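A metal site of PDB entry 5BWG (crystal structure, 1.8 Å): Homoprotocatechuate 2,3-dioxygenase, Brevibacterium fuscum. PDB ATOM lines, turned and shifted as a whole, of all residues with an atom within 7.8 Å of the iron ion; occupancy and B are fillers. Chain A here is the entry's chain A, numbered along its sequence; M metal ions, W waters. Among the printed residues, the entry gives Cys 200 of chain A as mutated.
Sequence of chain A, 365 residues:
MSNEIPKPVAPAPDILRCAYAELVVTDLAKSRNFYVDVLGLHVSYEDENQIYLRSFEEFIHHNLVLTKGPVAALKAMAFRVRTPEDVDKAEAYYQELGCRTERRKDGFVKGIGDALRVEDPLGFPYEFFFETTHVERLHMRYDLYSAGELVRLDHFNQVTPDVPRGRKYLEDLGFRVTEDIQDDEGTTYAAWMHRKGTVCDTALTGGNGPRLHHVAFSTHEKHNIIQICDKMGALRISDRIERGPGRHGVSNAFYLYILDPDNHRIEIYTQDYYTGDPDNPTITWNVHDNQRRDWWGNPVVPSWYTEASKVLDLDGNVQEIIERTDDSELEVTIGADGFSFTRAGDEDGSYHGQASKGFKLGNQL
OE2 of Glu 267 sits at hydrogen-bond distance from OH of Tyr 257 (3.3 Å).
The backbone NH (N) of Asn 157 sits at hydrogen-bond distance from the backbone carbonyl oxygen (O) of His 214, 3.0 Å away.
OE2 of Glu 267 sits at hydrogen-bond distance from NE2 of His 248, 2.8 Å away.
A ring nitrogen (ND1) of His 214 lies within hydrogen-bond range of a ring nitrogen (ND1) of His 213 (2.9 Å).
A ring nitrogen (ND1) of His 155 sits at hydrogen-bond distance from the side-chain carboxylate (OD2) of Asp 154 (2.7 Å).
The backbone NH (N) of Glu 267 sits at hydrogen-bond distance from the backbone carbonyl oxygen (O) of Val 215, at 2.9 Å.
The backbone carbonyl oxygen of His 155 sits at hydrogen-bond distance from the backbone NH of Ala 216, 2.8 Å away.
Along chain A the residues within 4 Å of the iron ion span positions 155 to 267.
The iron ion is bound by the side-chain carboxylate (OE1) of Glu 267, water W2, water W1, a ring nitrogen (NE2) of His 155, a ring nitrogen (NE2) of His 214 and water W3.
Water W1 lies within hydrogen-bond range of the indole nitrogen (NE1) of Trp 192 (2.9 Å) and the side-chain amide nitrogen (ND2) of Asn 157 (2.9 Å).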
ATOM      1  N   ASP A 154     -27.797  -0.873  27.236  1.00  0.00           N
ATOM      2  CA  ASP A 154     -28.881  -1.001  26.234  1.00  0.00           C
ATOM      3  C   ASP A 154     -28.393  -1.586  24.885  1.00  0.00           C
ATOM      4  O   ASP A 154     -29.046  -2.509  24.362  1.00  0.00           O
ATOM      5  CB  ASP A 154     -29.618   0.290  25.974  1.00  0.00           C
ATOM      6  CG  ASP A 154     -30.893   0.040  25.114  1.00  0.00           C
ATOM      7  OD1 ASP A 154     -31.912  -0.460  25.673  1.00  0.00           O
ATOM      8  OD2 ASP A 154     -30.869   0.264  23.860  1.00  0.00           O
ATOM      9  N   HIS A 155     -27.337  -1.030  24.314  1.00  0.00           N
ATOM     10  CA  HIS A 155     -26.926  -1.427  22.952  1.00  0.00           C
ATOM     11  C   HIS A 155     -25.532  -1.011  22.588  1.00  0.00           C
ATOM     12  O   HIS A 155     -24.964  -0.167  23.255  1.00  0.00           O
ATOM     13  CB  HIS A 155     -27.903  -0.936  21.852  1.00  0.00           C
ATOM     14  CG  HIS A 155     -27.976   0.558  21.676  1.00  0.00           C
ATOM     15  ND1 HIS A 155     -28.880   1.334  22.351  1.00  0.00           N
ATOM     16  CD2 HIS A 155     -27.295   1.412  20.860  1.00  0.00           C
ATOM     17  CE1 HIS A 155     -28.760   2.598  21.975  1.00  0.00           C
ATOM     18  NE2 HIS A 155     -27.789   2.682  21.088  1.00  0.00           N
ATOM     19  N   PHE A 156     -25.042  -1.587  21.490  1.00  0.00           N
ATOM     20  CA  PHE A 156     -23.839  -1.155  20.789  1.00  0.00           C
ATOM     21  C   PHE A 156     -24.248  -0.521  19.448  1.00  0.00           C
ATOM     22  O   PHE A 156     -25.351  -0.793  18.933  1.00  0.00           O
ATOM     23  CB  PHE A 156     -22.922  -2.347  20.482  1.00  0.00           C
ATOM     24  CG  PHE A 156     -22.628  -3.264  21.667  1.00  0.00           C
ATOM     25  CD1 PHE A 156     -22.124  -2.773  22.863  1.00  0.00           C
ATOM     26  CD2 PHE A 156     -22.860  -4.646  21.566  1.00  0.00           C
ATOM     27  CE1 PHE A 156     -21.840  -3.629  23.930  1.00  0.00           C
ATOM     28  CE2 PHE A 156     -22.611  -5.492  22.634  1.00  0.00           C
ATOM     29  CZ  PHE A 156     -22.105  -4.986  23.810  1.00  0.00           C
ATOM     30  N   ASN A 157     -23.368   0.315  18.875  1.00  0.00           N
ATOM     31  CA  ASN A 157     -23.570   0.792  17.516  1.00  0.00           C
ATOM     32  C   ASN A 157     -22.224   0.734  16.800  1.00  0.00           C
ATOM     33  O   ASN A 157     -21.245   1.257  17.270  1.00  0.00           O
ATOM     34  CB  ASN A 157     -24.167   2.203  17.541  1.00  0.00           C
ATOM     35  CG  ASN A 157     -24.469   2.743  16.183  1.00  0.00           C
ATOM     36  OD1 ASN A 157     -23.591   2.759  15.300  1.00  0.00           O
ATOM     37  ND2 ASN A 157     -25.720   3.210  15.975  1.00  0.00           N
ATOM     38  N   TRP A 192     -30.991  -0.506  12.622  1.00  0.00           N
ATOM     39  CA  TRP A 192     -31.015  -0.919  14.010  1.00  0.00           C
ATOM     40  C   TRP A 192     -31.633  -2.300  14.111  1.00  0.00           C
ATOM     41  O   TRP A 192     -32.606  -2.581  13.451  1.00  0.00           O
ATOM     42  CB  TRP A 192     -31.825   0.086  14.822  1.00  0.00           C
ATOM     43  CG  TRP A 192     -31.102   1.424  15.062  1.00  0.00           C
ATOM     44  CD1 TRP A 192     -30.478   1.844  16.218  1.00  0.00           C
ATOM     45  CD2 TRP A 192     -30.942   2.509  14.127  1.00  0.00           C
ATOM     46  NE1 TRP A 192     -29.936   3.102  16.052  1.00  0.00           N
ATOM     47  CE2 TRP A 192     -30.207   3.539  14.781  1.00  0.00           C
ATOM     48  CE3 TRP A 192     -31.339   2.709  12.799  1.00  0.00           C
ATOM     49  CZ2 TRP A 192     -29.890   4.755  14.151  1.00  0.00           C
ATOM     50  CZ3 TRP A 192     -31.001   3.911  12.151  1.00  0.00           C
ATOM     51  CH2 TRP A 192     -30.299   4.925  12.831  1.00  0.00           C
ATOM     52  N   CYS A 200     -32.868  -1.735  19.793  1.00  0.00           N
ATOM     53  CA  CYS A 200     -31.695  -2.455  19.410  1.00  0.00           C
ATOM     54  C   CYS A 200     -30.831  -3.057  20.497  1.00  0.00           C
ATOM     55  O   CYS A 200     -30.928  -2.750  21.678  1.00  0.00           O
ATOM     56  CB  CYS A 200     -30.891  -1.688  18.383  1.00  0.00           C
ATOM     57  SG  CYS A 200     -29.720  -0.531  19.057  1.00  0.00           S
ATOM     58  N   ALA A 203     -26.381  -1.992  16.240  1.00  0.00           N
ATOM     59  CA  ALA A 203     -26.849  -1.120  15.169  1.00  0.00           C
ATOM     60  C   ALA A 203     -25.677  -0.926  14.228  1.00  0.00           C
ATOM     61  O   ALA A 203     -24.516  -1.073  14.622  1.00  0.00           O
ATOM     62  CB  ALA A 203     -27.368   0.219  15.702  1.00  0.00           C
ATOM     63  N   THR A 205     -23.992   1.687  11.475  1.00  0.00           N
ATOM     64  CA  THR A 205     -23.905   3.046  10.959  1.00  0.00           C
ATOM     65  C   THR A 205     -22.984   2.977   9.766  1.00  0.00           C
ATOM     66  O   THR A 205     -21.859   2.458   9.855  1.00  0.00           O
ATOM     67  CB  THR A 205     -23.388   4.049  11.997  1.00  0.00           C
ATOM     68  OG1 THR A 205     -24.298   4.116  13.082  1.00  0.00           O
ATOM     69  CG2 THR A 205     -23.168   5.423  11.367  1.00  0.00           C
ATOM     70  N   HIS A 213     -19.053   2.835  17.064  1.00  0.00           N
ATOM     71  CA  HIS A 213     -19.580   4.148  17.144  1.00  0.00           C
ATOM     72  C   HIS A 213     -19.844   4.577  18.589  1.00  0.00           C
ATOM     73  O   HIS A 213     -19.407   5.654  19.010  1.00  0.00           O
ATOM     74  CB  HIS A 213     -20.856   4.320  16.308  1.00  0.00           C
ATOM     75  CG  HIS A 213     -21.142   5.742  16.034  1.00  0.00           C
ATOM     76  ND1 HIS A 213     -21.767   6.549  16.949  1.00  0.00           N
ATOM     77  CD2 HIS A 213     -20.807   6.550  14.990  1.00  0.00           C
ATOM     78  CE1 HIS A 213     -21.815   7.775  16.499  1.00  0.00           C
ATOM     79  NE2 HIS A 213     -21.267   7.805  15.290  1.00  0.00           N
ATOM     80  N   HIS A 214     -20.579   3.752  19.300  1.00  0.00           N
ATOM     81  CA  HIS A 214     -20.836   4.006  20.707  1.00  0.00           C
ATOM     82  C   HIS A 214     -21.330   2.791  21.434  1.00  0.00           C
ATOM     83  O   HIS A 214     -21.735   1.783  20.848  1.00  0.00           O
ATOM     84  CB  HIS A 214     -21.818   5.181  20.886  1.00  0.00           C
ATOM     85  CG  HIS A 214     -23.175   4.978  20.270  1.00  0.00           C
ATOM     86  ND1 HIS A 214     -23.504   5.481  19.024  1.00  0.00           N
ATOM     87  CD2 HIS A 214     -24.298   4.399  20.749  1.00  0.00           C
ATOM     88  CE1 HIS A 214     -24.756   5.200  18.760  1.00  0.00           C
ATOM     89  NE2 HIS A 214     -25.251   4.524  19.770  1.00  0.00           N
ATOM     90  N   VAL A 215     -21.331   2.930  22.761  1.00  0.00           N
ATOM     91  CA  VAL A 215     -21.998   2.031  23.661  1.00  0.00           C
ATOM     92  C   VAL A 215     -23.081   2.826  24.356  1.00  0.00           C
ATOM     93  O   VAL A 215     -22.845   3.941  24.742  1.00  0.00           O
ATOM     94  CB  VAL A 215     -20.977   1.536  24.720  1.00  0.00           C
ATOM     95  CG1 VAL A 215     -21.663   0.699  25.757  1.00  0.00           C
ATOM     96  CG2 VAL A 215     -19.866   0.727  24.052  1.00  0.00           C
ATOM     97  N   ALA A 216     -24.263   2.245  24.534  1.00  0.00           N
ATOM     98  CA  ALA A 216     -25.340   2.990  25.105  1.00  0.00           C
ATOM     99  C   ALA A 216     -25.777   2.409  26.429  1.00  0.00           C
ATOM    100  O   ALA A 216     -26.013   1.187  26.534  1.00  0.00           O
ATOM    101  CB  ALA A 216     -26.539   3.072  24.135  1.00  0.00           C
ATOM    102  N   HIS A 248     -34.659  11.227  19.767  1.00  0.00           N
ATOM    103  CA  HIS A 248     -34.381  10.620  18.475  1.00  0.00           C
ATOM    104  C   HIS A 248     -35.676  10.528  17.655  1.00  0.00           C
ATOM    105  O   HIS A 248     -36.782  10.385  18.216  1.00  0.00           O
ATOM    106  CB  HIS A 248     -33.857   9.196  18.614  1.00  0.00           C
ATOM    107  CG  HIS A 248     -32.417   9.089  19.014  1.00  0.00           C
ATOM    108  ND1 HIS A 248     -31.384   9.681  18.310  1.00  0.00           N
ATOM    109  CD2 HIS A 248     -31.829   8.360  19.995  1.00  0.00           C
ATOM    110  CE1 HIS A 248     -30.227   9.342  18.852  1.00  0.00           C
ATOM    111  NE2 HIS A 248     -30.475   8.554  19.875  1.00  0.00           N
ATOM    112  N   VAL A 250     -35.502   8.018  14.890  1.00  0.00           N
ATOM    113  CA  VAL A 250     -35.233   6.600  14.976  1.00  0.00           C
ATOM    114  C   VAL A 250     -35.126   6.192  16.447  1.00  0.00           C
ATOM    115  O   VAL A 250     -34.292   6.709  17.153  1.00  0.00           O
ATOM    116  CB  VAL A 250     -33.891   6.239  14.325  1.00  0.00           C
ATOM    117  CG1 VAL A 250     -33.560   4.780  14.655  1.00  0.00           C
ATOM    118  CG2 VAL A 250     -34.003   6.434  12.808  1.00  0.00           C
ATOM    119  N   SER A 251     -35.972   5.270  16.876  1.00  0.00           N
ATOM    120  CA  SER A 251     -36.019   4.740  18.293  1.00  0.00           C
ATOM    121  C   SER A 251     -36.980   5.487  19.178  1.00  0.00           C
ATOM    122  O   SER A 251     -37.382   4.950  20.201  1.00  0.00           O
ATOM    123  CB  SER A 251     -34.651   4.624  18.983  1.00  0.00           C
ATOM    124  OG  SER A 251     -34.178   5.867  19.524  1.00  0.00           O
ATOM    125  N   TYR A 255     -32.041  11.048  24.400  1.00  0.00           N
ATOM    126  CA  TYR A 255     -30.650  10.673  24.235  1.00  0.00           C
ATOM    127  C   TYR A 255     -29.683  11.791  24.546  1.00  0.00           C
ATOM    128  O   TYR A 255     -30.061  12.976  24.605  1.00  0.00           O
ATOM    129  CB  TYR A 255     -30.393  10.202  22.790  1.00  0.00           C
ATOM    130  CG  TYR A 255     -30.360  11.321  21.785  1.00  0.00           C
ATOM    131  CD1 TYR A 255     -29.196  12.030  21.533  1.00  0.00           C
ATOM    132  CD2 TYR A 255     -31.513  11.694  21.081  1.00  0.00           C
ATOM    133  CE1 TYR A 255     -29.154  13.071  20.578  1.00  0.00           C
ATOM    134  CE2 TYR A 255     -31.489  12.723  20.156  1.00  0.00           C
ATOM    135  CZ  TYR A 255     -30.326  13.418  19.924  1.00  0.00           C
ATOM    136  OH  TYR A 255     -30.331  14.417  18.981  1.00  0.00           O
ATOM    137  N   TYR A 257     -25.100  12.140  23.770  1.00  0.00           N
ATOM    138  CA  TYR A 257     -23.775  11.540  23.454  1.00  0.00           C
ATOM    139  C   TYR A 257     -22.662  12.346  24.107  1.00  0.00           C
ATOM    140  O   TYR A 257     -22.582  13.575  23.951  1.00  0.00           O
ATOM    141  CB  TYR A 257     -23.527  11.549  21.937  1.00  0.00           C
ATOM    142  CG  TYR A 257     -24.536  10.758  21.164  1.00  0.00           C
ATOM    143  CD1 TYR A 257     -24.424   9.391  21.045  1.00  0.00           C
ATOM    144  CD2 TYR A 257     -25.632  11.377  20.575  1.00  0.00           C
ATOM    145  CE1 TYR A 257     -25.383   8.626  20.376  1.00  0.00           C
ATOM    146  CE2 TYR A 257     -26.588  10.642  19.867  1.00  0.00           C
ATOM    147  CZ  TYR A 257     -26.455   9.276  19.760  1.00  0.00           C
ATOM    148  OH  TYR A 257     -27.387   8.558  19.083  1.00  0.00           O
ATOM    149  N   GLU A 267     -23.492   6.778  24.624  1.00  0.00           N
ATOM    150  CA  GLU A 267     -24.857   7.337  24.549  1.00  0.00           C
ATOM    151  C   GLU A 267     -25.546   7.057  25.879  1.00  0.00           C
ATOM    152  O   GLU A 267     -25.433   5.946  26.399  1.00  0.00           O
ATOM    153  CB  GLU A 267     -25.641   6.658  23.435  1.00  0.00           C
ATOM    154  CG  GLU A 267     -27.020   7.259  23.187  1.00  0.00           C
ATOM    155  CD  GLU A 267     -27.759   6.619  22.024  1.00  0.00           C
ATOM    156  OE1 GLU A 267     -27.288   5.595  21.489  1.00  0.00           O
ATOM    157  OE2 GLU A 267     -28.838   7.134  21.644  1.00  0.00           O
ATOM    158  N   ILE A 268     -26.353   8.019  26.348  1.00  0.00           N
ATOM    159  CA  ILE A 268     -27.282   7.807  27.417  1.00  0.00           C
ATOM    160  C   ILE A 268     -28.667   7.891  26.800  1.00  0.00           C
ATOM    161  O   ILE A 268     -28.877   8.737  25.969  1.00  0.00           O
ATOM    162  CB  ILE A 268     -27.101   8.867  28.524  1.00  0.00           C
ATOM    163  CG1 ILE A 268     -25.636   9.196  28.802  1.00  0.00           C
ATOM    164  CG2 ILE A 268     -27.746   8.411  29.817  1.00  0.00           C
ATOM    165  CD1 ILE A 268     -24.809   8.086  29.330  1.00  0.00           C
ATOM    166  N   TYR A 269     -29.563   6.980  27.152  1.00  0.00           N
ATOM    167  CA  TYR A 269     -30.739   6.640  26.369  1.00  0.00           C
ATOM    168  C   TYR A 269     -31.896   6.328  27.289  1.00  0.00           C
ATOM    169  O   TYR A 269     -31.724   5.726  28.329  1.00  0.00           O
ATOM    170  CB  TYR A 269     -30.336   5.394  25.572  1.00  0.00           C
ATOM    171  CG  TYR A 269     -31.239   4.796  24.552  1.00  0.00           C
ATOM    172  CD1 TYR A 269     -31.193   5.191  23.218  1.00  0.00           C
ATOM    173  CD2 TYR A 269     -32.042   3.688  24.891  1.00  0.00           C
ATOM    174  CE1 TYR A 269     -31.955   4.569  22.250  1.00  0.00           C
ATOM    175  CE2 TYR A 269     -32.824   3.072  23.926  1.00  0.00           C
ATOM    176  CZ  TYR A 269     -32.759   3.510  22.610  1.00  0.00           C
ATOM    177  OH  TYR A 269     -33.499   2.890  21.655  1.00  0.00           O
ATOM    178  N   ARG A 293     -32.936  11.848  13.051  1.00  0.00           N
ATOM    179  CA  ARG A 293     -31.943  11.603  14.081  1.00  0.00           C
ATOM    180  C   ARG A 293     -32.214  12.408  15.337  1.00  0.00           C
ATOM    181  O   ARG A 293     -32.194  11.845  16.412  1.00  0.00           O
ATOM    182  CB  ARG A 293     -30.540  11.871  13.550  1.00  0.00           C
ATOM    183  CG  ARG A 293     -30.076  10.765  12.613  1.00  0.00           C
ATOM    184  CD  ARG A 293     -28.578  10.741  12.451  1.00  0.00           C
ATOM    185  NE  ARG A 293     -28.140   9.620  11.622  1.00  0.00           N
ATOM    186  CZ  ARG A 293     -28.000   8.367  12.018  1.00  0.00           C
ATOM    187  NH1 ARG A 293     -28.241   7.985  13.278  1.00  0.00           N
ATOM    188  NH2 ARG A 293     -27.516   7.487  11.147  1.00  0.00           N
ATOM    189  N   TRP A 304     -19.960  13.603  14.898  1.00  0.00           N
ATOM    190  CA  TRP A 304     -20.814  12.464  15.205  1.00  0.00           C
ATOM    191  C   TRP A 304     -20.767  11.470  14.060  1.00  0.00           C
ATOM    192  O   TRP A 304     -20.829  10.243  14.279  1.00  0.00           O
ATOM    193  CB  TRP A 304     -22.260  12.905  15.542  1.00  0.00           C
ATOM    194  CG  TRP A 304     -23.075  11.839  16.192  1.00  0.00           C
ATOM    195  CD1 TRP A 304     -23.208  11.623  17.517  1.00  0.00           C
ATOM    196  CD2 TRP A 304     -23.805  10.806  15.547  1.00  0.00           C
ATOM    197  NE1 TRP A 304     -24.007  10.537  17.750  1.00  0.00           N
ATOM    198  CE2 TRP A 304     -24.379  10.007  16.543  1.00  0.00           C
ATOM    199  CE3 TRP A 304     -24.051  10.479  14.208  1.00  0.00           C
ATOM    200  CZ2 TRP A 304     -25.170   8.904  16.254  1.00  0.00           C
ATOM    201  CZ3 TRP A 304     -24.818   9.387  13.934  1.00  0.00           C
ATOM    202  CH2 TRP A 304     -25.370   8.619  14.954  1.00  0.00           C
HETATM  203 FE    FE M   1     -27.470   4.423  19.764  1.00  0.00          FE
HETATM  204  O   HOH W   1     -27.792   3.113  18.045  1.00  0.00           O
HETATM  205  O   HOH W   2     -29.596   4.910  19.880  1.00  0.00           O
HETATM  206  O   HOH W   3     -27.567   6.250  18.347  1.00  0.00           O
